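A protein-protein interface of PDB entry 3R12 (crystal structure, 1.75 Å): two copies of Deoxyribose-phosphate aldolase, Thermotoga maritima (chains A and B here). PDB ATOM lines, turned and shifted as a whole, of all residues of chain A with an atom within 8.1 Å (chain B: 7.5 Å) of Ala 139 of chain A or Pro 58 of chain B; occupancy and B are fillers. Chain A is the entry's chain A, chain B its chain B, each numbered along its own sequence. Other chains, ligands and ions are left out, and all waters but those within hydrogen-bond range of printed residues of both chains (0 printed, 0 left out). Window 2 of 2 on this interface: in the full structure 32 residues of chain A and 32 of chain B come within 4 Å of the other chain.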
ATOM      1  N   HIS A  11      -1.991 -16.827  -4.876  1.00  0.00           N
ATOM      2  CA  HIS A  11      -1.904 -16.392  -6.275  1.00  0.00           C
ATOM      3  C   HIS A  11      -0.957 -15.183  -6.377  1.00  0.00           C
ATOM      4  O   HIS A  11      -0.063 -15.139  -7.221  1.00  0.00           O
ATOM      5  CB  HIS A  11      -3.286 -15.995  -6.784  1.00  0.00           C
ATOM      6  CG  HIS A  11      -3.283 -15.301  -8.118  1.00  0.00           C
ATOM      7  ND1 HIS A  11      -3.650 -15.938  -9.284  1.00  0.00           N
ATOM      8  CD2 HIS A  11      -2.997 -14.018  -8.464  1.00  0.00           C
ATOM      9  CE1 HIS A  11      -3.557 -15.093 -10.295  1.00  0.00           C
ATOM     10  NE2 HIS A  11      -3.163 -13.920  -9.825  1.00  0.00           N
ATOM     11  N   ASN A 133      -1.554 -27.707 -17.198  1.00  0.00           N
ATOM     12  CA  ASN A 133      -2.712 -27.127 -17.834  1.00  0.00           C
ATOM     13  C   ASN A 133      -2.270 -25.862 -18.538  1.00  0.00           C
ATOM     14  O   ASN A 133      -2.190 -24.772 -17.927  1.00  0.00           O
ATOM     15  CB  ASN A 133      -3.872 -26.880 -16.835  1.00  0.00           C
ATOM     16  CG  ASN A 133      -5.175 -26.614 -17.544  1.00  0.00           C
ATOM     17  OD1 ASN A 133      -5.229 -25.736 -18.409  1.00  0.00           O
ATOM     18  ND2 ASN A 133      -6.225 -27.383 -17.216  1.00  0.00           N
ATOM     19  N   VAL A 134      -1.979 -26.015 -19.830  1.00  0.00           N
ATOM     20  CA  VAL A 134      -1.398 -24.945 -20.630  1.00  0.00           C
ATOM     21  C   VAL A 134      -2.334 -23.728 -20.753  1.00  0.00           C
ATOM     22  O   VAL A 134      -1.896 -22.592 -20.638  1.00  0.00           O
ATOM     23  CB  VAL A 134      -0.987 -25.458 -22.057  1.00  0.00           C
ATOM     24  CG1 VAL A 134      -0.522 -24.330 -22.934  1.00  0.00           C
ATOM     25  CG2 VAL A 134       0.100 -26.567 -21.952  1.00  0.00           C
ATOM     26  N   GLY A 135      -3.610 -23.991 -21.024  1.00  0.00           N
ATOM     27  CA  GLY A 135      -4.626 -22.958 -21.151  1.00  0.00           C
ATOM     28  C   GLY A 135      -4.772 -22.096 -19.906  1.00  0.00           C
ATOM     29  O   GLY A 135      -4.844 -20.862 -19.990  1.00  0.00           O
ATOM     30  N   MET A 136      -4.762 -22.736 -18.737  1.00  0.00           N
ATOM     31  CA  MET A 136      -4.887 -21.989 -17.466  1.00  0.00           C
ATOM     32  C   MET A 136      -3.576 -21.230 -17.130  1.00  0.00           C
ATOM     33  O   MET A 136      -3.627 -20.147 -16.552  1.00  0.00           O
ATOM     34  CB  MET A 136      -5.289 -22.908 -16.306  1.00  0.00           C
ATOM     35  CG  MET A 136      -6.693 -23.527 -16.426  1.00  0.00           C
ATOM     36  SD  MET A 136      -8.063 -22.148 -16.291  1.00  0.00           S
ATOM     37  CE  MET A 136      -8.089 -21.964 -14.339  1.00  0.00           C
ATOM     38  N   LEU A 137      -2.421 -21.785 -17.515  1.00  0.00           N
ATOM     39  CA  LEU A 137      -1.162 -21.039 -17.417  1.00  0.00           C
ATOM     40  C   LEU A 137      -1.174 -19.763 -18.289  1.00  0.00           C
ATOM     41  O   LEU A 137      -0.820 -18.675 -17.812  1.00  0.00           O
ATOM     42  CB  LEU A 137       0.042 -21.926 -17.787  1.00  0.00           C
ATOM     43  CG  LEU A 137       1.447 -21.302 -17.581  1.00  0.00           C
ATOM     44  CD1 LEU A 137       1.848 -21.312 -16.120  1.00  0.00           C
ATOM     45  CD2 LEU A 137       2.435 -22.104 -18.484  1.00  0.00           C
ATOM     46  N   LYS A 138      -1.601 -19.905 -19.546  1.00  0.00           N
ATOM     47  CA  LYS A 138      -1.738 -18.781 -20.467  1.00  0.00           C
ATOM     48  C   LYS A 138      -2.754 -17.735 -20.002  1.00  0.00           C
ATOM     49  O   LYS A 138      -2.590 -16.546 -20.280  1.00  0.00           O
ATOM     50  CB  LYS A 138      -2.083 -19.277 -21.876  1.00  0.00           C
ATOM     51  CG  LYS A 138      -0.949 -20.071 -22.548  1.00  0.00           C
ATOM     52  CD  LYS A 138      -1.183 -20.280 -24.033  1.00  0.00           C
ATOM     53  CE  LYS A 138      -0.770 -19.059 -24.862  1.00  0.00           C
ATOM     54  NZ  LYS A 138       0.741 -18.953 -25.105  1.00  0.00           N
ATOM     55  N   ALA A 139      -3.785 -18.182 -19.287  1.00  0.00           N
ATOM     56  CA  ALA A 139      -4.772 -17.296 -18.646  1.00  0.00           C
ATOM     57  C   ALA A 139      -4.258 -16.658 -17.329  1.00  0.00           C
ATOM     58  O   ALA A 139      -4.980 -15.916 -16.685  1.00  0.00           O
ATOM     59  CB  ALA A 139      -6.106 -18.057 -18.390  1.00  0.00           C
ATOM     60  N   LYS A 140      -3.024 -16.959 -16.940  1.00  0.00           N
ATOM     61  CA  LYS A 140      -2.384 -16.460 -15.706  1.00  0.00           C
ATOM     62  C   LYS A 140      -3.109 -16.895 -14.442  1.00  0.00           C
ATOM     63  O   LYS A 140      -3.135 -16.173 -13.450  1.00  0.00           O
ATOM     64  CB  LYS A 140      -2.245 -14.938 -15.737  1.00  0.00           C
ATOM     65  CG  LYS A 140      -1.466 -14.428 -16.919  1.00  0.00           C
ATOM     66  CD  LYS A 140      -1.181 -12.917 -16.804  1.00  0.00           C
ATOM     67  CE  LYS A 140      -0.001 -12.504 -17.655  1.00  0.00           C
ATOM     68  NZ  LYS A 140      -0.132 -12.979 -19.073  1.00  0.00           N
ATOM     69  N   GLU A 141      -3.691 -18.083 -14.485  1.00  0.00           N
ATOM     70  CA  GLU A 141      -4.397 -18.670 -13.350  1.00  0.00           C
ATOM     71  C   GLU A 141      -3.403 -19.499 -12.533  1.00  0.00           C
ATOM     72  O   GLU A 141      -3.470 -20.758 -12.453  1.00  0.00           O
ATOM     73  CB  GLU A 141      -5.566 -19.517 -13.858  1.00  0.00           C
ATOM     74  CG  GLU A 141      -6.568 -18.735 -14.714  1.00  0.00           C
ATOM     75  CD  GLU A 141      -7.544 -17.910 -13.930  1.00  0.00           C
ATOM     76  OE1 GLU A 141      -7.333 -17.713 -12.717  1.00  0.00           O
ATOM     77  OE2 GLU A 141      -8.534 -17.456 -14.541  1.00  0.00           O
ATOM     78  N   TRP A 142      -2.468 -18.759 -11.924  1.00  0.00           N
ATOM     79  CA  TRP A 142      -1.304 -19.336 -11.310  1.00  0.00           C
ATOM     80  C   TRP A 142      -1.700 -20.318 -10.203  1.00  0.00           C
ATOM     81  O   TRP A 142      -1.070 -21.358 -10.053  1.00  0.00           O
ATOM     82  CB  TRP A 142      -0.384 -18.268 -10.702  1.00  0.00           C
ATOM     83  CG  TRP A 142      -0.002 -17.099 -11.569  1.00  0.00           C
ATOM     84  CD1 TRP A 142      -0.016 -15.801 -11.194  1.00  0.00           C
ATOM     85  CD2 TRP A 142       0.450 -17.123 -12.920  1.00  0.00           C
ATOM     86  NE1 TRP A 142       0.426 -14.995 -12.216  1.00  0.00           N
ATOM     87  CE2 TRP A 142       0.716 -15.781 -13.294  1.00  0.00           C
ATOM     88  CE3 TRP A 142       0.668 -18.138 -13.858  1.00  0.00           C
ATOM     89  CZ2 TRP A 142       1.173 -15.435 -14.568  1.00  0.00           C
ATOM     90  CZ3 TRP A 142       1.138 -17.797 -15.111  1.00  0.00           C
ATOM     91  CH2 TRP A 142       1.377 -16.448 -15.457  1.00  0.00           C
ATOM     92  N   VAL A 145      -2.958 -23.591 -11.618  1.00  0.00           N
ATOM     93  CA  VAL A 145      -1.858 -24.350 -12.220  1.00  0.00           C
ATOM     94  C   VAL A 145      -0.996 -24.960 -11.111  1.00  0.00           C
ATOM     95  O   VAL A 145      -0.644 -26.146 -11.152  1.00  0.00           O
ATOM     96  CB  VAL A 145      -1.045 -23.435 -13.176  1.00  0.00           C
ATOM     97  CG1 VAL A 145       0.199 -24.135 -13.719  1.00  0.00           C
ATOM     98  CG2 VAL A 145      -1.910 -22.949 -14.299  1.00  0.00           C
ATOM     99  N   GLU A 174       5.816 -17.142 -20.084  1.00  0.00           N
ATOM    100  CA  GLU A 174       5.035 -18.313 -19.678  1.00  0.00           C
ATOM    101  C   GLU A 174       5.904 -19.520 -19.434  1.00  0.00           C
ATOM    102  O   GLU A 174       5.632 -20.301 -18.533  1.00  0.00           O
ATOM    103  CB  GLU A 174       4.005 -18.655 -20.726  1.00  0.00           C
ATOM    104  CG  GLU A 174       2.937 -17.603 -20.788  1.00  0.00           C
ATOM    105  CD  GLU A 174       2.139 -17.678 -22.065  1.00  0.00           C
ATOM    106  OE1 GLU A 174       2.600 -18.303 -23.050  1.00  0.00           O
ATOM    107  OE2 GLU A 174       1.043 -17.094 -22.060  1.00  0.00           O
ATOM    108  N   PHE B  55      -4.305 -25.321 -25.235  1.00  0.00           N
ATOM    109  CA  PHE B  55      -4.004 -23.929 -24.901  1.00  0.00           C
ATOM    110  C   PHE B  55      -5.289 -23.072 -24.762  1.00  0.00           C
ATOM    111  O   PHE B  55      -5.241 -21.867 -24.580  1.00  0.00           O
ATOM    112  CB  PHE B  55      -3.015 -23.336 -25.926  1.00  0.00           C
ATOM    113  CG  PHE B  55      -3.400 -23.559 -27.372  1.00  0.00           C
ATOM    114  CD1 PHE B  55      -4.374 -22.770 -27.980  1.00  0.00           C
ATOM    115  CD2 PHE B  55      -2.785 -24.551 -28.129  1.00  0.00           C
ATOM    116  CE1 PHE B  55      -4.734 -22.981 -29.314  1.00  0.00           C
ATOM    117  CE2 PHE B  55      -3.124 -24.742 -29.466  1.00  0.00           C
ATOM    118  CZ  PHE B  55      -4.077 -23.954 -30.056  1.00  0.00           C
ATOM    119  N   ALA B  56      -6.446 -23.710 -24.830  1.00  0.00           N
ATOM    120  CA  ALA B  56      -7.727 -23.036 -24.686  1.00  0.00           C
ATOM    121  C   ALA B  56      -7.851 -22.422 -23.286  1.00  0.00           C
ATOM    122  O   ALA B  56      -7.606 -23.085 -22.276  1.00  0.00           O
ATOM    123  CB  ALA B  56      -8.887 -24.048 -24.941  1.00  0.00           C
ATOM    124  N   THR B  57      -8.258 -21.160 -23.223  1.00  0.00           N
ATOM    125  CA  THR B  57      -8.410 -20.438 -21.957  1.00  0.00           C
ATOM    126  C   THR B  57      -9.892 -20.367 -21.521  1.00  0.00           C
ATOM    127  O   THR B  57     -10.771 -20.589 -22.345  1.00  0.00           O
ATOM    128  CB  THR B  57      -7.923 -19.005 -22.139  1.00  0.00           C
ATOM    129  OG1 THR B  57      -8.738 -18.368 -23.130  1.00  0.00           O
ATOM    130  CG2 THR B  57      -6.427 -18.976 -22.569  1.00  0.00           C
ATOM    131  N   PRO B  58     -10.168 -20.007 -20.246  1.00  0.00           N
ATOM    132  CA  PRO B  58     -11.581 -19.773 -19.891  1.00  0.00           C
ATOM    133  C   PRO B  58     -12.287 -18.823 -20.854  1.00  0.00           C
ATOM    134  O   PRO B  58     -13.426 -19.046 -21.207  1.00  0.00           O
ATOM    135  CB  PRO B  58     -11.506 -19.156 -18.492  1.00  0.00           C
ATOM    136  CG  PRO B  58     -10.245 -19.747 -17.901  1.00  0.00           C
ATOM    137  CD  PRO B  58      -9.276 -19.811 -19.090  1.00  0.00           C
ATOM    138  N   ASP B  59     -11.630 -17.769 -21.279  1.00  0.00           N
ATOM    139  CA  ASP B  59     -12.268 -16.849 -22.222  1.00  0.00           C
ATOM    140  C   ASP B  59     -12.614 -17.498 -23.556  1.00  0.00           C
ATOM    141  O   ASP B  59     -13.684 -17.182 -24.175  1.00  0.00           O
ATOM    142  CB  ASP B  59     -11.376 -15.609 -22.432  1.00  0.00           C
ATOM    143  CG  ASP B  59     -11.449 -14.638 -21.254  1.00  0.00           C
ATOM    144  OD1 ASP B  59     -12.372 -14.745 -20.413  1.00  0.00           O
ATOM    145  OD2 ASP B  59     -10.563 -13.772 -21.160  1.00  0.00           O
ATOM    146  N   ASP B  60     -11.740 -18.391 -24.019  1.00  0.00           N
ATOM    147  CA  ASP B  60     -12.007 -19.127 -25.271  1.00  0.00           C
ATOM    148  C   ASP B  60     -13.258 -19.991 -25.125  1.00  0.00           C
ATOM    149  O   ASP B  60     -14.030 -20.128 -26.068  1.00  0.00           O
ATOM    150  CB  ASP B  60     -10.849 -20.030 -25.669  1.00  0.00           C
ATOM    151  CG  ASP B  60      -9.627 -19.272 -26.083  1.00  0.00           C
ATOM    152  OD1 ASP B  60      -9.757 -18.152 -26.628  1.00  0.00           O
ATOM    153  OD2 ASP B  60      -8.539 -19.811 -25.857  1.00  0.00           O
ATOM    154  N   ILE B  61     -13.427 -20.595 -23.955  1.00  0.00           N
ATOM    155  CA  ILE B  61     -14.579 -21.467 -23.671  1.00  0.00           C
ATOM    156  C   ILE B  61     -15.868 -20.629 -23.551  1.00  0.00           C
ATOM    157  O   ILE B  61     -16.943 -21.017 -24.021  1.00  0.00           O
ATOM    158  CB  ILE B  61     -14.363 -22.287 -22.368  1.00  0.00           C
ATOM    159  CG1 ILE B  61     -13.116 -23.183 -22.489  1.00  0.00           C
ATOM    160  CG2 ILE B  61     -15.621 -23.108 -22.039  1.00  0.00           C
ATOM    161  CD1 ILE B  61     -13.073 -24.006 -23.786  1.00  0.00           C
ATOM    162  N   LYS B  62     -15.752 -19.450 -22.931  1.00  0.00           N
ATOM    163  CA  LYS B  62     -16.884 -18.509 -22.867  1.00  0.00           C
ATOM    164  C   LYS B  62     -17.324 -18.136 -24.281  1.00  0.00           C
ATOM    165  O   LYS B  62     -18.518 -18.142 -24.568  1.00  0.00           O
ATOM    166  CB  LYS B  62     -16.526 -17.255 -22.065  1.00  0.00           C
ATOM    167  CG  LYS B  62     -16.423 -17.541 -20.577  1.00  0.00           C
ATOM    168  CD  LYS B  62     -15.879 -16.353 -19.819  1.00  0.00           C
ATOM    169  CE  LYS B  62     -15.695 -16.659 -18.339  1.00  0.00           C
ATOM    170  NZ  LYS B  62     -15.747 -15.379 -17.577  1.00  0.00           N
ATOM    171  N   LYS B  63     -16.356 -17.893 -25.174  1.00  0.00           N
ATOM    172  CA  LYS B  63     -16.654 -17.545 -26.571  1.00  0.00           C
ATOM    173  C   LYS B  63     -17.347 -18.712 -27.314  1.00  0.00           C
ATOM    174  O   LYS B  63     -18.311 -18.522 -28.052  1.00  0.00           O
ATOM    175  CB  LYS B  63     -15.352 -17.160 -27.280  1.00  0.00           C
ATOM    176  CG  LYS B  63     -15.514 -16.788 -28.724  1.00  0.00           C
ATOM    177  CD  LYS B  63     -14.187 -16.358 -29.331  1.00  0.00           C
ATOM    178  CE  LYS B  63     -14.124 -16.622 -30.852  1.00  0.00           C
ATOM    179  NZ  LYS B  63     -13.986 -18.077 -31.180  1.00  0.00           N
ATOM    180  N   LEU B  64     -16.826 -19.912 -27.115  1.00  0.00           N
ATOM    181  CA  LEU B  64     -17.418 -21.151 -27.693  1.00  0.00           C
ATOM    182  C   LEU B  64     -18.876 -21.329 -27.287  1.00  0.00           C
ATOM    183  O   LEU B  64     -19.733 -21.655 -28.114  1.00  0.00           O
ATOM    184  CB  LEU B  64     -16.618 -22.360 -27.224  1.00  0.00           C
ATOM    185  CG  LEU B  64     -16.892 -23.684 -27.899  1.00  0.00           C
ATOM    186  CD1 LEU B  64     -16.239 -23.703 -29.294  1.00  0.00           C
ATOM    187  CD2 LEU B  64     -16.369 -24.837 -27.010  1.00  0.00           C
ATOM    188  N   TYR B  82     -12.883 -27.860 -18.100  1.00  0.00           N
ATOM    189  CA  TYR B  82     -13.823 -26.799 -18.424  1.00  0.00           C
ATOM    190  C   TYR B  82     -15.298 -27.159 -18.434  1.00  0.00           C
ATOM    191  O   TYR B  82     -16.110 -26.330 -18.804  1.00  0.00           O
ATOM    192  CB  TYR B  82     -13.448 -26.218 -19.791  1.00  0.00           C
ATOM    193  CG  TYR B  82     -12.155 -25.406 -19.803  1.00  0.00           C
ATOM    194  CD1 TYR B  82     -11.877 -24.491 -18.810  1.00  0.00           C
ATOM    195  CD2 TYR B  82     -11.190 -25.586 -20.825  1.00  0.00           C
ATOM    196  CE1 TYR B  82     -10.685 -23.743 -18.803  1.00  0.00           C
ATOM    197  CE2 TYR B  82     -10.003 -24.851 -20.832  1.00  0.00           C
ATOM    198  CZ  TYR B  82      -9.762 -23.901 -19.822  1.00  0.00           C
ATOM    199  OH  TYR B  82      -8.587 -23.130 -19.815  1.00  0.00           O
ATOM    200  N   LEU B  85     -17.363 -24.766 -16.088  1.00  0.00           N
ATOM    201  CA  LEU B  85     -17.451 -23.457 -16.755  1.00  0.00           C
ATOM    202  C   LEU B  85     -18.489 -23.470 -17.877  1.00  0.00           C
ATOM    203  O   LEU B  85     -19.321 -22.565 -17.985  1.00  0.00           O
ATOM    204  CB  LEU B  85     -16.051 -23.038 -17.302  1.00  0.00           C
ATOM    205  CG  LEU B  85     -15.913 -21.731 -18.092  1.00  0.00           C
ATOM    206  CD1 LEU B  85     -16.364 -20.590 -17.189  1.00  0.00           C
ATOM    207  CD2 LEU B  85     -14.494 -21.531 -18.591  1.00  0.00           C
ATOM    208  N   GLU B  89     -21.824 -21.361 -18.084  1.00  0.00           N
ATOM    209  CA  GLU B  89     -22.047 -20.477 -19.212  1.00  0.00           C
ATOM    210  C   GLU B  89     -23.323 -20.770 -20.009  1.00  0.00           C
ATOM    211  O   GLU B  89     -23.870 -19.863 -20.654  1.00  0.00           O
ATOM    212  CB  GLU B  89     -20.848 -20.476 -20.153  1.00  0.00           C
ATOM    213  CG  GLU B  89     -19.555 -19.862 -19.538  1.00  0.00           C
ATOM    214  CD  GLU B  89     -19.642 -18.392 -19.225  1.00  0.00           C
ATOM    215  OE1 GLU B  89     -20.064 -17.646 -20.095  1.00  0.00           O
ATOM    216  OE2 GLU B  89     -19.284 -17.978 -18.116  1.00  0.00           O
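The side-chain sulfur (SD) of Met 136 of chain A lies within hydrogen-bond range of the side-chain hydroxyl (OH) of Tyr 82 of chain B (3.7 Å).
The side-chain amide oxygen (OD1) of Asn 133 of chain A is in hydrogen-bond range of the backbone NH (N) of Met 136 of chain A (3.1 Å).
N of Glu 141 of chain A sits at hydrogen-bond distance from O of Met 136 of chain A.
The backbone carbonyl oxygen of Ala 56 of chain B sits at hydrogen-bond distance from the side-chain hydroxyl of Tyr 82 of chain B (2.6 Å).
The side-chain hydroxyl (OG1) of Thr 57 of chain B sits close to the backbone NH (N) of Asp 59 of chain B.
The side-chain carboxylate of Asp 60 of chain B sits at hydrogen-bond distance from the backbone NH of Thr 57 of chain B, 3.0 Å away.
Among the printed residues, pairs that only touch across the chains: Gly 135 of chain A with Ala 56 of chain B, Gly 135 of chain A with Thr 57 of chain B, Met 136 of chain A with Pro 58 of chain B, Gly 135 of chain A with Phe 55 of chain B, Ala 139 of chain A with Pro 58 of chain B and Gly 135 of chain A with Tyr 82 of chain B.
Asn 133 of chain A touches none of the printed residues of chain B.
Of the printed residues of chain B, Met 136 of chain A touches Pro 58 and Tyr 82.
Ala 139 of chain A touches just one residue of chain B: Pro 58 (3.7 Å).
Printed residues of chain A within 4 Å of Ala 56 of chain B: Gly 135.
Lys 63 of chain B touches none of the printed residues of chain A.
The nearest residue of chain A that does not touch Pro 58 of chain B is Glu 141 of chain A (4.4 Å).
Hydrophobic or aromatic side chains of chain A within 4 Å of the printed part of chain B: Met 136 and Ala 139.
Of the 13 printed residues of chain B, 5 touch a printed residue of chain A.
Printed residues of chain B that touch a printed residue of chain A: Phe 55, Ala 56, Thr 57, Pro 58 and Tyr 82.
Among the printed residues, no Asp or Glu carboxylate lies within 4 Å of a Lys or Arg side-chain nitrogen of the other chain.
No position is printed for both chains.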
